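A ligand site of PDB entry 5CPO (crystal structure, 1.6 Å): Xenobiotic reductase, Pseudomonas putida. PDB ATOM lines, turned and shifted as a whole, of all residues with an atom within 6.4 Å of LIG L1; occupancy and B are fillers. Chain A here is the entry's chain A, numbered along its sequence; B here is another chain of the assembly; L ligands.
An oxygen (O4) of LG2 L2 lies within hydrogen-bond range of the guanidinium group (NH2) of Arg 231, 2.8 Å away. The backbone NH (N) of Cys 25 is in hydrogen-bond range of an oxygen (O2) of LG2 L2. The backbone NH of Trp 302 lies within hydrogen-bond range of an oxygen (O6) of LG2 L2 (3.1 Å). An oxygen (O3) of LG2 L2 sits at hydrogen-bond distance from the backbone carbonyl oxygen of Pro 23 (2.8 Å). An oxygen (O2) of LG2 L2 sits at hydrogen-bond distance from the backbone NH (N) of Ala 57 (3.0 Å). A nitrogen (N3) of LG2 L2 is in hydrogen-bond range of the side-chain amide oxygen of Gln 99. ND1 of His 181 lies close to O1 of LG2 L2, 3.5 Å away. An oxygen (O1) of LIG L1 sits at hydrogen-bond distance from a ring nitrogen (NE2) of His 178, at 2.8 Å. ND1 of His 181 sits at hydrogen-bond distance from O1 of LIG L1 (2.7 Å). O2 of LG2 L2 sits at hydrogen-bond distance from SG of Cys 25, at 3.3 Å. A nitrogen (N2) of LIG L1 is in hydrogen-bond range of the side-chain sulfur of Cys 25, 3.6 Å away. A ring nitrogen (NE2) of His 178 is in hydrogen-bond range of an oxygen (O1) of LG2 L2 (3.3 Å).
The backbone NH of Ala 180 is in hydrogen-bond range of a ring nitrogen (ND1) of His 178, 3.3 Å away. The side-chain amino group (NZ) of Lys 106 sits at hydrogen-bond distance from the backbone carbonyl oxygen (O) of His 181 (3.1 Å). The side-chain amide oxygen of Gln 99 sits close to the backbone NH of Ala 57, 3.4 Å away. O of Phe 269 lies within hydrogen-bond range of NZ of Lys 106 (2.9 Å).
An oxygen (O1) of LIG L1 lies close to a nitrogen (N2) of LG2 L2, 3.2 Å away.
Merely in contact with LIG L1: Tyr 183, Trp 302, Ile 66, Tyr 27, Phe 269, Ala 57 and Trp 358 of chain B. Within 4 Å of LIG L1: Cys 25, Tyr 27, Ala 57, Ile 66, His 178, His 181, Tyr 183, Phe 269, Trp 302 and Trp 358 of chain B. The nearest printed residue that does not touch LIG L1 is Lys 106 (4.8 Å).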
ATOM      1  N   PRO A  23       2.007   8.958 -19.316  1.00  0.00           N
ATOM      2  CA  PRO A  23       1.631  10.355 -19.095  1.00  0.00           C
ATOM      3  C   PRO A  23       0.272  10.475 -18.393  1.00  0.00           C
ATOM      4  O   PRO A  23      -0.672   9.790 -18.789  1.00  0.00           O
ATOM      5  CB  PRO A  23       1.609  10.938 -20.536  1.00  0.00           C
ATOM      6  CG  PRO A  23       1.334   9.736 -21.431  1.00  0.00           C
ATOM      7  CD  PRO A  23       2.112   8.631 -20.757  1.00  0.00           C
ATOM      8  N   CYS A  25      -1.961  13.787 -17.106  1.00  0.00           N
ATOM      9  CA  CYS A  25      -2.312  15.199 -16.855  1.00  0.00           C
ATOM     10  C   CYS A  25      -2.680  15.440 -15.408  1.00  0.00           C
ATOM     11  O   CYS A  25      -3.482  14.707 -14.837  1.00  0.00           O
ATOM     12  CB  CYS A  25      -3.500  15.618 -17.711  1.00  0.00           C
ATOM     13  SG  CYS A  25      -3.089  15.841 -19.452  1.00  0.00           S
ATOM     14  N   TYR A  27      -3.394  18.858 -14.474  1.00  0.00           N
ATOM     15  CA  TYR A  27      -4.250  20.055 -14.539  1.00  0.00           C
ATOM     16  C   TYR A  27      -3.911  21.108 -13.469  1.00  0.00           C
ATOM     17  O   TYR A  27      -4.792  21.840 -13.004  1.00  0.00           O
ATOM     18  CB  TYR A  27      -5.738  19.666 -14.448  1.00  0.00           C
ATOM     19  CG  TYR A  27      -6.158  18.529 -15.365  1.00  0.00           C
ATOM     20  CD1 TYR A  27      -6.575  18.773 -16.672  1.00  0.00           C
ATOM     21  CD2 TYR A  27      -6.138  17.211 -14.924  1.00  0.00           C
ATOM     22  CE1 TYR A  27      -6.955  17.740 -17.504  1.00  0.00           C
ATOM     23  CE2 TYR A  27      -6.504  16.183 -15.755  1.00  0.00           C
ATOM     24  CZ  TYR A  27      -6.917  16.461 -17.048  1.00  0.00           C
ATOM     25  OH  TYR A  27      -7.261  15.434 -17.867  1.00  0.00           O
ATOM     26  N   ALA A  57       0.814  14.862 -20.921  1.00  0.00           N
ATOM     27  CA  ALA A  57       0.560  15.589 -22.160  1.00  0.00           C
ATOM     28  C   ALA A  57       0.905  17.076 -22.004  1.00  0.00           C
ATOM     29  O   ALA A  57       0.306  17.803 -21.201  1.00  0.00           O
ATOM     30  CB  ALA A  57      -0.885  15.437 -22.598  1.00  0.00           C
ATOM     31  N   ILE A  66      -5.501  20.870 -23.263  1.00  0.00           N
ATOM     32  CA  ILE A  66      -6.882  20.390 -23.077  1.00  0.00           C
ATOM     33  C   ILE A  66      -7.640  21.447 -22.263  1.00  0.00           C
ATOM     34  O   ILE A  66      -8.768  21.803 -22.594  1.00  0.00           O
ATOM     35  CB  ILE A  66      -6.952  19.011 -22.356  1.00  0.00           C
ATOM     36  CG1 ILE A  66      -6.121  17.948 -23.081  1.00  0.00           C
ATOM     37  CG2 ILE A  66      -8.413  18.531 -22.236  1.00  0.00           C
ATOM     38  CD1 ILE A  66      -5.866  16.708 -22.229  1.00  0.00           C
ATOM     39  N   GLN A  99       5.531  13.382 -23.024  1.00  0.00           N
ATOM     40  CA  GLN A  99       4.556  13.333 -24.096  1.00  0.00           C
ATOM     41  C   GLN A  99       4.205  14.745 -24.590  1.00  0.00           C
ATOM     42  O   GLN A  99       3.731  15.575 -23.796  1.00  0.00           O
ATOM     43  CB  GLN A  99       3.295  12.608 -23.623  1.00  0.00           C
ATOM     44  CG  GLN A  99       2.287  12.400 -24.730  1.00  0.00           C
ATOM     45  CD  GLN A  99       0.952  11.917 -24.214  1.00  0.00           C
ATOM     46  OE1 GLN A  99       0.294  12.596 -23.416  1.00  0.00           O
ATOM     47  NE2 GLN A  99       0.538  10.727 -24.663  1.00  0.00           N
ATOM     48  N   LYS A 106     -10.822  18.633 -28.832  1.00  0.00           N
ATOM     49  CA  LYS A 106     -11.140  18.393 -27.427  1.00  0.00           C
ATOM     50  C   LYS A 106     -10.514  19.439 -26.518  1.00  0.00           C
ATOM     51  O   LYS A 106     -10.635  19.341 -25.298  1.00  0.00           O
ATOM     52  CB  LYS A 106     -10.706  16.981 -27.019  1.00  0.00           C
ATOM     53  CG  LYS A 106     -11.430  15.888 -27.825  1.00  0.00           C
ATOM     54  CD  LYS A 106     -10.934  14.474 -27.524  1.00  0.00           C
ATOM     55  CE  LYS A 106     -11.881  13.730 -26.606  1.00  0.00           C
ATOM     56  NZ  LYS A 106     -11.645  12.244 -26.607  1.00  0.00           N
ATOM     57  N   PRO A 112     -11.209  18.155 -15.033  1.00  0.00           N
ATOM     58  CA  PRO A 112     -12.190  17.061 -14.870  1.00  0.00           C
ATOM     59  C   PRO A 112     -13.087  17.209 -13.628  1.00  0.00           C
ATOM     60  O   PRO A 112     -14.262  16.847 -13.682  1.00  0.00           O
ATOM     61  CB  PRO A 112     -11.313  15.815 -14.744  1.00  0.00           C
ATOM     62  CG  PRO A 112     -10.084  16.157 -15.539  1.00  0.00           C
ATOM     63  CD  PRO A 112      -9.849  17.630 -15.255  1.00  0.00           C
ATOM     64  N   HIS A 178       1.872  12.471 -29.022  1.00  0.00           N
ATOM     65  CA  HIS A 178       0.522  12.097 -28.617  1.00  0.00           C
ATOM     66  C   HIS A 178      -0.425  12.060 -29.822  1.00  0.00           C
ATOM     67  O   HIS A 178      -1.026  13.066 -30.170  1.00  0.00           O
ATOM     68  CB  HIS A 178      -0.024  13.072 -27.559  1.00  0.00           C
ATOM     69  CG  HIS A 178      -1.210  12.548 -26.831  1.00  0.00           C
ATOM     70  ND1 HIS A 178      -1.879  11.390 -27.223  1.00  0.00           N
ATOM     71  CD2 HIS A 178      -1.845  12.983 -25.713  1.00  0.00           C
ATOM     72  CE1 HIS A 178      -2.862  11.164 -26.370  1.00  0.00           C
ATOM     73  NE2 HIS A 178      -2.856  12.105 -25.438  1.00  0.00           N
ATOM     74  N   ALA A 180      -2.997   9.919 -29.926  1.00  0.00           N
ATOM     75  CA  ALA A 180      -4.099   9.110 -29.435  1.00  0.00           C
ATOM     76  C   ALA A 180      -5.237   9.917 -28.779  1.00  0.00           C
ATOM     77  O   ALA A 180      -5.209  11.140 -28.720  1.00  0.00           O
ATOM     78  CB  ALA A 180      -3.566   8.060 -28.423  1.00  0.00           C
ATOM     79  N   HIS A 181      -6.246   9.168 -28.312  1.00  0.00           N
ATOM     80  CA  HIS A 181      -7.300   9.686 -27.424  1.00  0.00           C
ATOM     81  C   HIS A 181      -8.140  10.814 -28.005  1.00  0.00           C
ATOM     82  O   HIS A 181      -8.727  11.608 -27.264  1.00  0.00           O
ATOM     83  CB  HIS A 181      -6.659  10.115 -26.098  1.00  0.00           C
ATOM     84  CG  HIS A 181      -5.944   9.002 -25.408  1.00  0.00           C
ATOM     85  ND1 HIS A 181      -5.124   9.195 -24.322  1.00  0.00           N
ATOM     86  CD2 HIS A 181      -5.919   7.665 -25.665  1.00  0.00           C
ATOM     87  CE1 HIS A 181      -4.629   8.023 -23.932  1.00  0.00           C
ATOM     88  NE2 HIS A 181      -5.103   7.081 -24.736  1.00  0.00           N
ATOM     89  N   GLY A 182      -8.227  10.874 -29.336  1.00  0.00           N
ATOM     90  CA  GLY A 182      -9.170  11.788 -29.967  1.00  0.00           C
ATOM     91  C   GLY A 182      -8.702  13.207 -30.146  1.00  0.00           C
ATOM     92  O   GLY A 182      -9.464  14.050 -30.649  1.00  0.00           O
ATOM     93  N   TYR A 183      -7.456  13.484 -29.756  1.00  0.00           N
ATOM     94  CA  TYR A 183      -6.837  14.791 -29.893  1.00  0.00           C
ATOM     95  C   TYR A 183      -6.386  14.964 -31.347  1.00  0.00           C
ATOM     96  O   TYR A 183      -6.834  14.205 -32.213  1.00  0.00           O
ATOM     97  CB  TYR A 183      -5.698  14.916 -28.873  1.00  0.00           C
ATOM     98  CG  TYR A 183      -6.209  14.725 -27.461  1.00  0.00           C
ATOM     99  CD1 TYR A 183      -7.209  15.553 -26.941  1.00  0.00           C
ATOM    100  CD2 TYR A 183      -5.748  13.686 -26.660  1.00  0.00           C
ATOM    101  CE1 TYR A 183      -7.705  15.372 -25.651  1.00  0.00           C
ATOM    102  CE2 TYR A 183      -6.250  13.499 -25.350  1.00  0.00           C
ATOM    103  CZ  TYR A 183      -7.233  14.347 -24.872  1.00  0.00           C
ATOM    104  OH  TYR A 183      -7.712  14.132 -23.586  1.00  0.00           O
ATOM    105  N   ARG A 231       2.126   7.557 -29.059  1.00  0.00           N
ATOM    106  CA  ARG A 231       0.937   6.889 -28.560  1.00  0.00           C
ATOM    107  C   ARG A 231      -0.144   7.038 -29.615  1.00  0.00           C
ATOM    108  O   ARG A 231      -0.307   8.105 -30.195  1.00  0.00           O
ATOM    109  CB  ARG A 231       0.480   7.477 -27.202  1.00  0.00           C
ATOM    110  CG  ARG A 231      -0.573   6.612 -26.504  1.00  0.00           C
ATOM    111  CD  ARG A 231      -0.816   7.024 -25.068  1.00  0.00           C
ATOM    112  NE  ARG A 231      -1.087   5.839 -24.244  1.00  0.00           N
ATOM    113  CZ  ARG A 231      -1.333   5.879 -22.935  1.00  0.00           C
ATOM    114  NH1 ARG A 231      -1.391   7.055 -22.305  1.00  0.00           N
ATOM    115  NH2 ARG A 231      -1.537   4.749 -22.269  1.00  0.00           N
ATOM    116  N   PHE A 269     -10.801   6.889 -28.733  1.00  0.00           N
ATOM    117  CA  PHE A 269     -11.681   7.896 -28.103  1.00  0.00           C
ATOM    118  C   PHE A 269     -12.015   9.066 -29.040  1.00  0.00           C
ATOM    119  O   PHE A 269     -12.145  10.196 -28.610  1.00  0.00           O
ATOM    120  CB  PHE A 269     -11.042   8.460 -26.811  1.00  0.00           C
ATOM    121  CG  PHE A 269     -10.748   7.418 -25.778  1.00  0.00           C
ATOM    122  CD1 PHE A 269     -11.766   6.665 -25.209  1.00  0.00           C
ATOM    123  CD2 PHE A 269      -9.455   7.192 -25.345  1.00  0.00           C
ATOM    124  CE1 PHE A 269     -11.482   5.710 -24.253  1.00  0.00           C
ATOM    125  CE2 PHE A 269      -9.184   6.233 -24.389  1.00  0.00           C
ATOM    126  CZ  PHE A 269     -10.191   5.494 -23.843  1.00  0.00           C
ATOM    127  N   TRP A 278     -14.119  -2.116 -21.173  1.00  0.00           N
ATOM    128  CA  TRP A 278     -13.230  -1.908 -20.044  1.00  0.00           C
ATOM    129  C   TRP A 278     -13.095  -3.165 -19.208  1.00  0.00           C
ATOM    130  O   TRP A 278     -14.082  -3.808 -18.881  1.00  0.00           O
ATOM    131  CB  TRP A 278     -13.746  -0.776 -19.144  1.00  0.00           C
ATOM    132  CG  TRP A 278     -13.989   0.490 -19.848  1.00  0.00           C
ATOM    133  CD1 TRP A 278     -15.189   1.054 -20.120  1.00  0.00           C
ATOM    134  CD2 TRP A 278     -12.996   1.393 -20.343  1.00  0.00           C
ATOM    135  NE1 TRP A 278     -15.007   2.255 -20.770  1.00  0.00           N
ATOM    136  CE2 TRP A 278     -13.675   2.479 -20.924  1.00  0.00           C
ATOM    137  CE3 TRP A 278     -11.595   1.380 -20.358  1.00  0.00           C
ATOM    138  CZ2 TRP A 278     -13.004   3.547 -21.504  1.00  0.00           C
ATOM    139  CZ3 TRP A 278     -10.942   2.434 -20.947  1.00  0.00           C
ATOM    140  CH2 TRP A 278     -11.639   3.508 -21.517  1.00  0.00           C
ATOM    141  N   TRP A 302      -4.235   0.607 -19.060  1.00  0.00           N
ATOM    142  CA  TRP A 302      -5.684   0.431 -18.943  1.00  0.00           C
ATOM    143  C   TRP A 302      -5.954  -0.917 -18.294  1.00  0.00           C
ATOM    144  O   TRP A 302      -6.500  -1.831 -18.924  1.00  0.00           O
ATOM    145  CB  TRP A 302      -6.419   0.532 -20.299  1.00  0.00           C
ATOM    146  CG  TRP A 302      -6.157   1.795 -21.097  1.00  0.00           C
ATOM    147  CD1 TRP A 302      -5.322   1.944 -22.192  1.00  0.00           C
ATOM    148  CD2 TRP A 302      -6.733   3.074 -20.870  1.00  0.00           C
ATOM    149  NE1 TRP A 302      -5.370   3.230 -22.640  1.00  0.00           N
ATOM    150  CE2 TRP A 302      -6.219   3.956 -21.845  1.00  0.00           C
ATOM    151  CE3 TRP A 302      -7.647   3.566 -19.946  1.00  0.00           C
ATOM    152  CZ2 TRP A 302      -6.574   5.280 -21.905  1.00  0.00           C
ATOM    153  CZ3 TRP A 302      -7.998   4.900 -20.008  1.00  0.00           C
ATOM    154  CH2 TRP A 302      -7.471   5.739 -20.985  1.00  0.00           C
ATOM    155  N   TRP B 358      -9.728  10.810  -9.817  1.00  0.00           N
ATOM    156  CA  TRP B 358      -9.563   9.638 -10.654  1.00  0.00           C
ATOM    157  C   TRP B 358      -9.685   8.328  -9.889  1.00  0.00           C
ATOM    158  O   TRP B 358      -9.960   7.273 -10.464  1.00  0.00           O
ATOM    159  CB  TRP B 358      -8.209   9.727 -11.364  1.00  0.00           C
ATOM    160  CG  TRP B 358      -8.136  10.935 -12.227  1.00  0.00           C
ATOM    161  CD1 TRP B 358      -7.534  12.127 -11.937  1.00  0.00           C
ATOM    162  CD2 TRP B 358      -8.702  11.088 -13.539  1.00  0.00           C
ATOM    163  NE1 TRP B 358      -7.689  13.000 -12.971  1.00  0.00           N
ATOM    164  CE2 TRP B 358      -8.386  12.393 -13.984  1.00  0.00           C
ATOM    165  CE3 TRP B 358      -9.430  10.255 -14.392  1.00  0.00           C
ATOM    166  CZ2 TRP B 358      -8.790  12.882 -15.212  1.00  0.00           C
ATOM    167  CZ3 TRP B 358      -9.816  10.733 -15.627  1.00  0.00           C
ATOM    168  CH2 TRP B 358      -9.494  12.041 -16.030  1.00  0.00           C
HETATM  169  C1  LIG L   1      -9.080  10.031 -23.188  1.00  0.00           C
HETATM  170  C2  LIG L   1     -10.021   9.251 -22.344  1.00  0.00           C
HETATM  171  C3  LIG L   1      -9.525   8.983 -20.904  1.00  0.00           C
HETATM  172  C4  LIG L   1      -8.001   9.012 -20.704  1.00  0.00           C
HETATM  173  N1  LIG L   1      -7.517  10.402 -20.530  1.00  0.00           N
HETATM  174  C5  LIG L   1      -6.561  10.793 -21.384  1.00  0.00           C
HETATM  175  C6  LIG L   1      -6.046  12.068 -21.340  1.00  0.00           C
HETATM  176  C7  LIG L   1      -6.504  12.980 -20.386  1.00  0.00           C
HETATM  177  C8  LIG L   1      -7.536  12.543 -19.499  1.00  0.00           C
HETATM  178  C9  LIG L   1      -8.007  11.226 -19.593  1.00  0.00           C
HETATM  179  C10 LIG L   1      -4.950  12.443 -22.334  1.00  0.00           C
HETATM  180  O1  LIG L   1      -4.626  11.678 -23.252  1.00  0.00           O
HETATM  181  N2  LIG L   1      -4.325  13.759 -22.136  1.00  0.00           N
HETATM  182  C1  LG2 L   2      -4.552   9.867 -18.104  1.00  0.00           C
HETATM  183  N1  LG2 L   2      -4.072   9.269 -19.357  1.00  0.00           N
HETATM  184  C2  LG2 L   2      -3.328  10.097 -20.305  1.00  0.00           C
HETATM  185  N2  LG2 L   2      -3.015   9.579 -21.473  1.00  0.00           N
HETATM  186  C3  LG2 L   2      -2.151  10.224 -22.277  1.00  0.00           C
HETATM  187  O1  LG2 L   2      -1.852   9.719 -23.326  1.00  0.00           O
HETATM  188  N3  LG2 L   2      -1.652  11.429 -21.886  1.00  0.00           N
HETATM  189  C4  LG2 L   2      -1.987  11.992 -20.718  1.00  0.00           C
HETATM  190  O2  LG2 L   2      -1.509  13.052 -20.383  1.00  0.00           O
HETATM  191  C5  LG2 L   2      -3.045  11.414 -20.041  1.00  0.00           C
HETATM  192  N4  LG2 L   2      -3.568  11.986 -18.818  1.00  0.00           N
HETATM  193  C6  LG2 L   2      -4.300  11.189 -17.843  1.00  0.00           C
HETATM  194  C7  LG2 L   2      -4.598  11.724 -16.576  1.00  0.00           C
HETATM  195  C8  LG2 L   2      -5.077  10.893 -15.587  1.00  0.00           C
HETATM  196  C9  LG2 L   2      -5.159  11.510 -14.196  1.00  0.00           C
HETATM  197  C10 LG2 L   2      -5.431   9.595 -15.910  1.00  0.00           C
HETATM  198  C11 LG2 L   2      -5.972   8.651 -14.834  1.00  0.00           C
HETATM  199  C12 LG2 L   2      -5.308   9.131 -17.204  1.00  0.00           C
HETATM  200  C13 LG2 L   2      -4.291   7.836 -19.616  1.00  0.00           C
HETATM  201  C14 LG2 L   2      -3.202   7.069 -18.847  1.00  0.00           C
HETATM  202  O3  LG2 L   2      -1.941   7.357 -19.395  1.00  0.00           O
HETATM  203  C15 LG2 L   2      -3.400   5.549 -18.823  1.00  0.00           C
HETATM  204  O4  LG2 L   2      -3.378   4.999 -20.129  1.00  0.00           O
HETATM  205  C16 LG2 L   2      -4.728   5.202 -18.127  1.00  0.00           C
HETATM  206  O5  LG2 L   2      -4.744   5.801 -16.850  1.00  0.00           O
HETATM  207  C17 LG2 L   2      -4.885   3.684 -18.009  1.00  0.00           C
HETATM  208  O6  LG2 L   2      -3.873   3.096 -17.238  1.00  0.00           O
HETATM  209  P1  LG2 L   2      -4.181   2.667 -15.666  1.00  0.00           P
HETATM  210  O7  LG2 L   2      -2.941   2.025 -15.132  1.00  0.00           O
HETATM  211  O8  LG2 L   2      -5.338   1.676 -15.626  1.00  0.00           O
HETATM  212  O9  LG2 L   2      -4.577   3.951 -14.937  1.00  0.00           O
